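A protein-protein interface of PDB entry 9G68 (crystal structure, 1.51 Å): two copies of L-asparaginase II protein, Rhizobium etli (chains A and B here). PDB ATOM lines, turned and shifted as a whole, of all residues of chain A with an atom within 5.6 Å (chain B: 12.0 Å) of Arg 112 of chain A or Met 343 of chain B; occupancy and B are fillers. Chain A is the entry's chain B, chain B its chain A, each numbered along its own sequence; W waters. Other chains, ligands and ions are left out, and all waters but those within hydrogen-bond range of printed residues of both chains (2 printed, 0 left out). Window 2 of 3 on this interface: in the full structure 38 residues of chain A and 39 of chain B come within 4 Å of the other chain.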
ATOM      1  N   ALA A 109      14.480 -15.490  -4.681  1.00  0.00           N
ATOM      2  CA  ALA A 109      13.094 -15.861  -4.939  1.00  0.00           C
ATOM      3  C   ALA A 109      12.408 -16.472  -3.726  1.00  0.00           C
ATOM      4  O   ALA A 109      11.176 -16.551  -3.713  1.00  0.00           O
ATOM      5  CB  ALA A 109      13.019 -16.821  -6.145  1.00  0.00           C
ATOM      6  N   ASP A 110      13.161 -16.876  -2.700  1.00  0.00           N
ATOM      7  CA  ASP A 110      12.596 -17.388  -1.458  1.00  0.00           C
ATOM      8  C   ASP A 110      12.174 -16.281  -0.500  1.00  0.00           C
ATOM      9  O   ASP A 110      11.464 -16.560   0.474  1.00  0.00           O
ATOM     10  CB  ASP A 110      13.615 -18.295  -0.764  1.00  0.00           C
ATOM     11  CG  ASP A 110      13.938 -19.526  -1.567  1.00  0.00           C
ATOM     12  OD1 ASP A 110      12.973 -20.190  -2.013  1.00  0.00           O
ATOM     13  OD2 ASP A 110      15.147 -19.837  -1.760  1.00  0.00           O
ATOM     14  N   LEU A 111      12.601 -15.041  -0.738  1.00  0.00           N
ATOM     15  CA  LEU A 111      12.210 -13.931   0.124  1.00  0.00           C
ATOM     16  C   LEU A 111      10.738 -13.608  -0.072  1.00  0.00           C
ATOM     17  O   LEU A 111      10.216 -13.667  -1.187  1.00  0.00           O
ATOM     18  CB  LEU A 111      13.055 -12.696  -0.172  1.00  0.00           C
ATOM     19  CG  LEU A 111      14.536 -12.845   0.168  1.00  0.00           C
ATOM     20  CD1 LEU A 111      15.352 -11.655  -0.344  1.00  0.00           C
ATOM     21  CD2 LEU A 111      14.737 -13.053   1.662  1.00  0.00           C
ATOM     22  N   ARG A 112      10.061 -13.283   1.027  1.00  0.00           N
ATOM     23  CA  ARG A 112       8.664 -12.864   0.982  1.00  0.00           C
ATOM     24  C   ARG A 112       8.486 -11.396   1.382  1.00  0.00           C
ATOM     25  O   ARG A 112       7.401 -10.998   1.810  1.00  0.00           O
ATOM     26  CB  ARG A 112       7.827 -13.793   1.867  1.00  0.00           C
ATOM     27  CG  ARG A 112       7.823 -15.234   1.364  1.00  0.00           C
ATOM     28  CD  ARG A 112       7.044 -15.343   0.067  1.00  0.00           C
ATOM     29  NE  ARG A 112       7.066 -16.704  -0.463  1.00  0.00           N
ATOM     30  CZ  ARG A 112       7.965 -17.148  -1.328  1.00  0.00           C
ATOM     31  NH1 ARG A 112       8.904 -16.352  -1.811  1.00  0.00           N
ATOM     32  NH2 ARG A 112       7.919 -18.423  -1.724  1.00  0.00           N
ATOM     33  N   CYS A 113       9.546 -10.596   1.275  1.00  0.00           N
ATOM     34  CA  CYS A 113       9.507  -9.150   1.419  1.00  0.00           C
ATOM     35  C   CYS A 113       9.635  -8.557   0.031  1.00  0.00           C
ATOM     36  O   CYS A 113      10.109  -9.221  -0.903  1.00  0.00           O
ATOM     37  CB  CYS A 113      10.636  -8.635   2.321  1.00  0.00           C
ATOM     38  SG  CYS A 113      12.283  -9.301   1.906  1.00  0.00           S
ATOM     39  N   GLY A 114       9.181  -7.316  -0.113  1.00  0.00           N
ATOM     40  CA  GLY A 114       9.219  -6.669  -1.411  1.00  0.00           C
ATOM     41  C   GLY A 114      10.108  -5.433  -1.424  1.00  0.00           C
ATOM     42  O   GLY A 114      10.443  -4.890  -0.366  1.00  0.00           O
ATOM     43  N   HIS A 145      14.505 -11.192   7.172  1.00  0.00           N
ATOM     44  CA  HIS A 145      13.869 -12.233   6.363  1.00  0.00           C
ATOM     45  C   HIS A 145      14.820 -13.388   6.082  1.00  0.00           C
ATOM     46  O   HIS A 145      14.414 -14.547   6.170  1.00  0.00           O
ATOM     47  CB  HIS A 145      13.325 -11.653   5.069  1.00  0.00           C
ATOM     48  CG  HIS A 145      12.042 -10.917   5.253  1.00  0.00           C
ATOM     49  ND1 HIS A 145      10.833 -11.436   4.848  1.00  0.00           N
ATOM     50  CD2 HIS A 145      11.767  -9.734   5.860  1.00  0.00           C
ATOM     51  CE1 HIS A 145       9.871 -10.584   5.153  1.00  0.00           C
ATOM     52  NE2 HIS A 145      10.408  -9.540   5.763  1.00  0.00           N
ATOM     53  N   THR A 159       9.776 -23.532   3.893  1.00  0.00           N
ATOM     54  CA  THR A 159      10.147 -22.134   3.736  1.00  0.00           C
ATOM     55  C   THR A 159       9.057 -21.293   3.092  1.00  0.00           C
ATOM     56  O   THR A 159       9.139 -20.069   3.196  1.00  0.00           O
ATOM     57  CB  THR A 159      11.432 -21.962   2.903  1.00  0.00           C
ATOM     58  OG1 THR A 159      11.342 -22.717   1.681  1.00  0.00           O
ATOM     59  CG2 THR A 159      12.657 -22.378   3.683  1.00  0.00           C
ATOM     60  N   ASP A 160       8.019 -21.898   2.488  1.00  0.00           N
ATOM     61  CA  ASP A 160       7.155 -21.109   1.611  1.00  0.00           C
ATOM     62  C   ASP A 160       6.396 -20.015   2.362  1.00  0.00           C
ATOM     63  O   ASP A 160       6.174 -18.926   1.802  1.00  0.00           O
ATOM     64  CB  ASP A 160       6.168 -21.991   0.846  1.00  0.00           C
ATOM     65  CG  ASP A 160       5.340 -21.180  -0.148  1.00  0.00           C
ATOM     66  OD1 ASP A 160       5.937 -20.422  -0.957  1.00  0.00           O
ATOM     67  OD2 ASP A 160       4.096 -21.278  -0.113  1.00  0.00           O
ATOM     68  N   GLY A 161       5.980 -20.272   3.597  1.00  0.00           N
ATOM     69  CA  GLY A 161       5.232 -19.305   4.368  1.00  0.00           C
ATOM     70  C   GLY A 161       5.914 -19.003   5.687  1.00  0.00           C
ATOM     71  O   GLY A 161       5.233 -18.806   6.709  1.00  0.00           O
ATOM     72  N   TYR A 162       7.258 -18.918   5.672  1.00  0.00           N
ATOM     73  CA  TYR A 162       8.038 -18.561   6.864  1.00  0.00           C
ATOM     74  C   TYR A 162       7.573 -17.259   7.516  1.00  0.00           C
ATOM     75  O   TYR A 162       7.811 -17.044   8.711  1.00  0.00           O
ATOM     76  CB  TYR A 162       9.532 -18.466   6.493  1.00  0.00           C
ATOM     77  CG  TYR A 162       9.944 -17.208   5.723  1.00  0.00           C
ATOM     78  CD1 TYR A 162      10.228 -16.013   6.387  1.00  0.00           C
ATOM     79  CD2 TYR A 162      10.055 -17.221   4.348  1.00  0.00           C
ATOM     80  CE1 TYR A 162      10.596 -14.875   5.694  1.00  0.00           C
ATOM     81  CE2 TYR A 162      10.408 -16.068   3.638  1.00  0.00           C
ATOM     82  CZ  TYR A 162      10.686 -14.915   4.318  1.00  0.00           C
ATOM     83  OH  TYR A 162      11.051 -13.793   3.619  1.00  0.00           O
ATOM     84  N   HIS A 163       6.904 -16.399   6.761  1.00  0.00           N
ATOM     85  CA  HIS A 163       6.484 -15.088   7.225  1.00  0.00           C
ATOM     86  C   HIS A 163       5.059 -15.074   7.759  1.00  0.00           C
ATOM     87  O   HIS A 163       4.615 -14.037   8.268  1.00  0.00           O
ATOM     88  CB  HIS A 163       6.601 -14.095   6.076  1.00  0.00           C
ATOM     89  CG  HIS A 163       5.695 -14.425   4.933  1.00  0.00           C
ATOM     90  ND1 HIS A 163       5.735 -15.637   4.269  1.00  0.00           N
ATOM     91  CD2 HIS A 163       4.714 -13.701   4.335  1.00  0.00           C
ATOM     92  CE1 HIS A 163       4.823 -15.642   3.315  1.00  0.00           C
ATOM     93  NE2 HIS A 163       4.195 -14.478   3.329  1.00  0.00           N
ATOM     94  N   GLY A 194       5.370  -3.347   6.722  1.00  0.00           N
ATOM     95  CA  GLY A 194       5.624  -3.051   5.319  1.00  0.00           C
ATOM     96  C   GLY A 194       6.431  -4.119   4.595  1.00  0.00           C
ATOM     97  O   GLY A 194       6.302  -4.281   3.374  1.00  0.00           O
ATOM     98  N   CYS A 195       7.277  -4.848   5.323  1.00  0.00           N
ATOM     99  CA  CYS A 195       8.042  -5.946   4.736  1.00  0.00           C
ATOM    100  C   CYS A 195       7.313  -7.282   4.831  1.00  0.00           C
ATOM    101  O   CYS A 195       7.916  -8.324   4.552  1.00  0.00           O
ATOM    102  CB  CYS A 195       9.423  -6.037   5.398  1.00  0.00           C
ATOM    103  SG  CYS A 195       9.336  -6.466   7.140  1.00  0.00           S
ATOM    104  N   ASN A 196       6.027  -7.262   5.207  1.00  0.00           N
ATOM    105  CA  ASN A 196       5.116  -8.393   5.156  1.00  0.00           C
ATOM    106  C   ASN A 196       5.299  -9.408   6.287  1.00  0.00           C
ATOM    107  O   ASN A 196       4.886 -10.582   6.135  1.00  0.00           O
ATOM    108  CB  ASN A 196       5.241  -9.095   3.812  1.00  0.00           C
ATOM    109  CG  ASN A 196       3.998  -9.773   3.410  1.00  0.00           C
ATOM    110  OD1 ASN A 196       2.893  -9.322   3.729  1.00  0.00           O
ATOM    111  ND2 ASN A 196       4.146 -10.882   2.713  1.00  0.00           N
ATOM    112  N   ARG B  18      -3.076   0.093  12.000  1.00  0.00           N
ATOM    113  CA  ARG B  18      -2.491  -1.064  11.337  1.00  0.00           C
ATOM    114  C   ARG B  18      -3.202  -2.278  11.923  1.00  0.00           C
ATOM    115  O   ARG B  18      -3.044  -2.578  13.111  1.00  0.00           O
ATOM    116  CB  ARG B  18      -0.978  -1.099  11.562  1.00  0.00           C
ATOM    117  CG  ARG B  18      -0.212  -2.204  10.801  1.00  0.00           C
ATOM    118  CD  ARG B  18       1.314  -2.004  10.984  1.00  0.00           C
ATOM    119  NE  ARG B  18       1.772  -0.753  10.366  1.00  0.00           N
ATOM    120  CZ  ARG B  18       2.105  -0.629   9.081  1.00  0.00           C
ATOM    121  NH1 ARG B  18       2.140  -1.684   8.275  1.00  0.00           N
ATOM    122  NH2 ARG B  18       2.375   0.588   8.588  1.00  0.00           N
ATOM    123  N   GLN B 338      -4.129   4.852   0.385  1.00  0.00           N
ATOM    124  CA  GLN B 338      -3.739   3.453   0.292  1.00  0.00           C
ATOM    125  C   GLN B 338      -2.843   3.052   1.456  1.00  0.00           C
ATOM    126  O   GLN B 338      -1.988   3.824   1.906  1.00  0.00           O
ATOM    127  CB  GLN B 338      -3.018   3.207  -1.030  1.00  0.00           C
ATOM    128  CG  GLN B 338      -3.929   3.310  -2.213  1.00  0.00           C
ATOM    129  CD  GLN B 338      -4.634   1.994  -2.521  1.00  0.00           C
ATOM    130  OE1 GLN B 338      -5.865   1.898  -2.432  1.00  0.00           O
ATOM    131  NE2 GLN B 338      -3.853   0.975  -2.902  1.00  0.00           N
ATOM    132  N   ARG B 339      -3.060   1.825   1.962  1.00  0.00           N
ATOM    133  CA  ARG B 339      -2.275   1.273   3.056  1.00  0.00           C
ATOM    134  C   ARG B 339      -1.979  -0.183   2.698  1.00  0.00           C
ATOM    135  O   ARG B 339      -2.515  -1.127   3.285  1.00  0.00           O
ATOM    136  CB  ARG B 339      -3.003   1.417   4.388  1.00  0.00           C
ATOM    137  CG  ARG B 339      -2.971   2.840   4.912  1.00  0.00           C
ATOM    138  CD  ARG B 339      -1.614   3.212   5.476  1.00  0.00           C
ATOM    139  NE  ARG B 339      -1.633   4.533   6.120  1.00  0.00           N
ATOM    140  CZ  ARG B 339      -1.549   5.688   5.468  1.00  0.00           C
ATOM    141  NH1 ARG B 339      -1.465   5.735   4.149  1.00  0.00           N
ATOM    142  NH2 ARG B 339      -1.552   6.829   6.160  1.00  0.00           N
ATOM    143  N   VAL B 340      -1.099  -0.346   1.712  1.00  0.00           N
ATOM    144  CA  VAL B 340      -0.763  -1.625   1.092  1.00  0.00           C
ATOM    145  C   VAL B 340       0.749  -1.792   1.154  1.00  0.00           C
ATOM    146  O   VAL B 340       1.491  -0.854   0.830  1.00  0.00           O
ATOM    147  CB  VAL B 340      -1.261  -1.674  -0.365  1.00  0.00           C
ATOM    148  CG1 VAL B 340      -0.707  -2.873  -1.096  1.00  0.00           C
ATOM    149  CG2 VAL B 340      -2.773  -1.700  -0.398  1.00  0.00           C
ATOM    150  N   ASN B 341       1.214  -2.976   1.577  1.00  0.00           N
ATOM    151  CA  ASN B 341       2.631  -3.096   1.874  1.00  0.00           C
ATOM    152  C   ASN B 341       3.393  -3.486   0.608  1.00  0.00           C
ATOM    153  O   ASN B 341       2.833  -3.543  -0.489  1.00  0.00           O
ATOM    154  CB  ASN B 341       2.869  -4.057   3.060  1.00  0.00           C
ATOM    155  CG  ASN B 341       2.539  -5.527   2.764  1.00  0.00           C
ATOM    156  OD1 ASN B 341       2.250  -5.923   1.632  1.00  0.00           O
ATOM    157  ND2 ASN B 341       2.601  -6.361   3.816  1.00  0.00           N
ATOM    158  N   THR B 342       4.698  -3.749   0.761  1.00  0.00           N
ATOM    159  CA  THR B 342       5.550  -4.078  -0.384  1.00  0.00           C
ATOM    160  C   THR B 342       5.196  -5.400  -1.054  1.00  0.00           C
ATOM    161  O   THR B 342       5.809  -5.732  -2.076  1.00  0.00           O
ATOM    162  CB  THR B 342       7.021  -4.146   0.017  1.00  0.00           C
ATOM    163  OG1 THR B 342       7.234  -5.257   0.907  1.00  0.00           O
ATOM    164  CG2 THR B 342       7.458  -2.855   0.675  1.00  0.00           C
ATOM    165  N   MET B 343       4.247  -6.170  -0.506  1.00  0.00           N
ATOM    166  CA  MET B 343       3.821  -7.429  -1.112  1.00  0.00           C
ATOM    167  C   MET B 343       2.350  -7.398  -1.530  1.00  0.00           C
ATOM    168  O   MET B 343       1.750  -8.455  -1.777  1.00  0.00           O
ATOM    169  CB  MET B 343       4.081  -8.585  -0.149  1.00  0.00           C
ATOM    170  CG  MET B 343       5.552  -8.844   0.126  1.00  0.00           C
ATOM    171  SD  MET B 343       6.369  -9.411  -1.369  1.00  0.00           S
ATOM    172  CE  MET B 343       5.887 -11.143  -1.448  1.00  0.00           C
ATOM    173  N   GLY B 344       1.754  -6.213  -1.588  1.00  0.00           N
ATOM    174  CA  GLY B 344       0.390  -6.055  -2.029  1.00  0.00           C
ATOM    175  C   GLY B 344      -0.674  -6.294  -0.983  1.00  0.00           C
ATOM    176  O   GLY B 344      -1.856  -6.335  -1.337  1.00  0.00           O
ATOM    177  N   VAL B 345      -0.304  -6.450   0.288  1.00  0.00           N
ATOM    178  CA  VAL B 345      -1.237  -6.800   1.356  1.00  0.00           C
ATOM    179  C   VAL B 345      -1.742  -5.507   1.992  1.00  0.00           C
ATOM    180  O   VAL B 345      -0.948  -4.598   2.259  1.00  0.00           O
ATOM    181  CB  VAL B 345      -0.541  -7.691   2.402  1.00  0.00           C
ATOM    182  CG1 VAL B 345      -1.487  -8.080   3.539  1.00  0.00           C
ATOM    183  CG2 VAL B 345       0.064  -8.923   1.746  1.00  0.00           C
ATOM    184  N   THR B 346      -3.055  -5.408   2.226  1.00  0.00           N
ATOM    185  CA  THR B 346      -3.613  -4.208   2.865  1.00  0.00           C
ATOM    186  C   THR B 346      -3.389  -4.327   4.366  1.00  0.00           C
ATOM    187  O   THR B 346      -3.805  -5.322   4.974  1.00  0.00           O
ATOM    188  CB  THR B 346      -5.100  -4.060   2.552  1.00  0.00           C
ATOM    189  OG1 THR B 346      -5.261  -3.802   1.152  1.00  0.00           O
ATOM    190  CG2 THR B 346      -5.700  -2.916   3.326  1.00  0.00           C
ATOM    191  N   THR B 347      -2.697  -3.348   4.955  1.00  0.00           N
ATOM    192  CA  THR B 347      -2.268  -3.451   6.339  1.00  0.00           C
ATOM    193  C   THR B 347      -3.045  -2.564   7.301  1.00  0.00           C
ATOM    194  O   THR B 347      -2.893  -2.734   8.520  1.00  0.00           O
ATOM    195  CB  THR B 347      -0.775  -3.081   6.488  1.00  0.00           C
ATOM    196  OG1 THR B 347      -0.593  -1.741   6.068  1.00  0.00           O
ATOM    197  CG2 THR B 347       0.155  -3.995   5.679  1.00  0.00           C
ATOM    198  N   GLY B 348      -3.809  -1.594   6.824  1.00  0.00           N
ATOM    199  CA  GLY B 348      -4.424  -0.663   7.752  1.00  0.00           C
ATOM    200  C   GLY B 348      -5.311   0.315   7.028  1.00  0.00           C
ATOM    201  O   GLY B 348      -5.726   0.061   5.903  1.00  0.00           O
HETATM  202  O   HOH W   1       9.062 -10.749  -3.097  1.00  0.00           O
HETATM  203  O   HOH W   2      10.157  -4.903   2.409  1.00  0.00           O
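The backbone NH (N) of Gly 114 of chain A is in hydrogen-bond range of the side-chain hydroxyl (OG1) of Thr 342 of chain B (3.0 Å).
The backbone carbonyl oxygen of Arg 112 of chain A lies close to the side-chain sulfur of Met 343 of chain B, at 3.7 Å.
SD of Met 343 of chain B lies close to O of Cys 113 of chain A, at 3.8 Å.
The backbone NH of Gly 114 of chain A sits at hydrogen-bond distance from the side-chain sulfur of Met 343 of chain B (3.7 Å).
The side-chain hydroxyl (OG1) of Thr 342 of chain B is in hydrogen-bond range of the backbone carbonyl oxygen (O) of Gly 194 of chain A (2.8 Å).
ND2 of Asn 341 of chain B sits at hydrogen-bond distance from OD1 of Asn 196 of chain A (3.0 Å).
The backbone carbonyl oxygen (O) of Arg 112 of chain A lies within hydrogen-bond range of the side-chain amide nitrogen (ND2) of Asn 196 of chain A, 3.4 Å away.
The backbone NH (N) of Gly 344 of chain B sits at hydrogen-bond distance from the side-chain amide oxygen (OD1) of Asn 341 of chain B (3.3 Å).
The backbone NH of Arg 112 of chain A sits at hydrogen-bond distance from the side-chain hydroxyl of Tyr 162 of chain A, at 2.8 Å.
O of Ala 109 of chain A is in hydrogen-bond range of NH1 of Arg 112 of chain A (3.0 Å).
NH2 of Arg 112 of chain A lies within salt-bridge range of OD1 of Asp 160 of chain A.
O of Cys 195 of chain A sits at hydrogen-bond distance from NE2 of His 145 of chain A (3.0 Å).
Among the printed residues, pairs that only touch across the chains: Gly 194 of chain A with Asn 341 of chain B, Asn 196 of chain A with Val 345 of chain B, Asn 196 of chain A with Met 343 of chain B, Gly 194 of chain A with Arg 18 of chain B and Cys 195 of chain A with Thr 342 of chain B.
No residue of chain B comes within 4 Å of Ala 109 of chain A.
No residue of chain B comes within 4 Å of Leu 111 of chain A.
Arg 112 of chain A touches one residue of chain B.
Of chain B, only Met 343 (3.7 Å) comes within 4 Å of Cys 113 of chain A.
No residue of chain B comes within 4 Å of His 145 of chain A.
Asp 160 of chain A touches none of the printed residues of chain B.
No residue of chain B comes within 4 Å of Gly 161 of chain A.
No residue of chain B comes within 4 Å of Tyr 162 of chain A.
No residue of chain B comes within 4 Å of His 163 of chain A.
Gly 194 of chain A touches just these residues of chain B: Arg 18 (3.95 Å), Asn 341 (3.5 Å) and Thr 342 (2.8 Å).
Of the printed residues of chain B, Asn 196 of chain A touches Asn 341 (3.0 Å), Met 343 (3.6 Å) and Val 345 (3.5 Å).
Of the printed residues of chain A, Arg 18 of chain B touches Gly 194.
Printed residues of chain A within 4 Å of Asn 341 of chain B: Gly 194 (3.5 Å) and Asn 196 (3.0 Å).
Of the printed residues of chain A, Thr 342 of chain B touches Gly 114, Gly 194 and Cys 195.
Met 343 of chain B touches four residues of chain A.
Printed residues of chain A within 4 Å of Val 345 of chain B: Asn 196.
Thr 346 of chain B touches none of the printed residues of chain A.
The nearest residue of chain B that does not touch Arg 112 of chain A is Thr 342 of chain B (5.8 Å).
Along chain A the printed residues that touch a printed residue of chain B span positions 112 to 196.
Hydrophobic or aromatic side chains of chain B that line the printed part of chain A: Met 343 and Val 345.
Among the printed residues, 11 pairs touch across the chains.
Among the printed residues, no Asp or Glu carboxylate lies within 4 Å of a Lys or Arg side-chain nitrogen of the other chain.
No position is printed for both chains.
Of the 11 pairs that touch across the chains among the printed residues, none has its exchanged pair printed and touching as well.
Water W2 bridges O of Gly 114 of chain A (2.8 Å) and OG1 of Thr 342 of chain B (3.3 Å).
Water W1 bridges O of Cys 113 of chain A (2.9 Å) and SD of Met 343 of chain B (3.5 Å).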
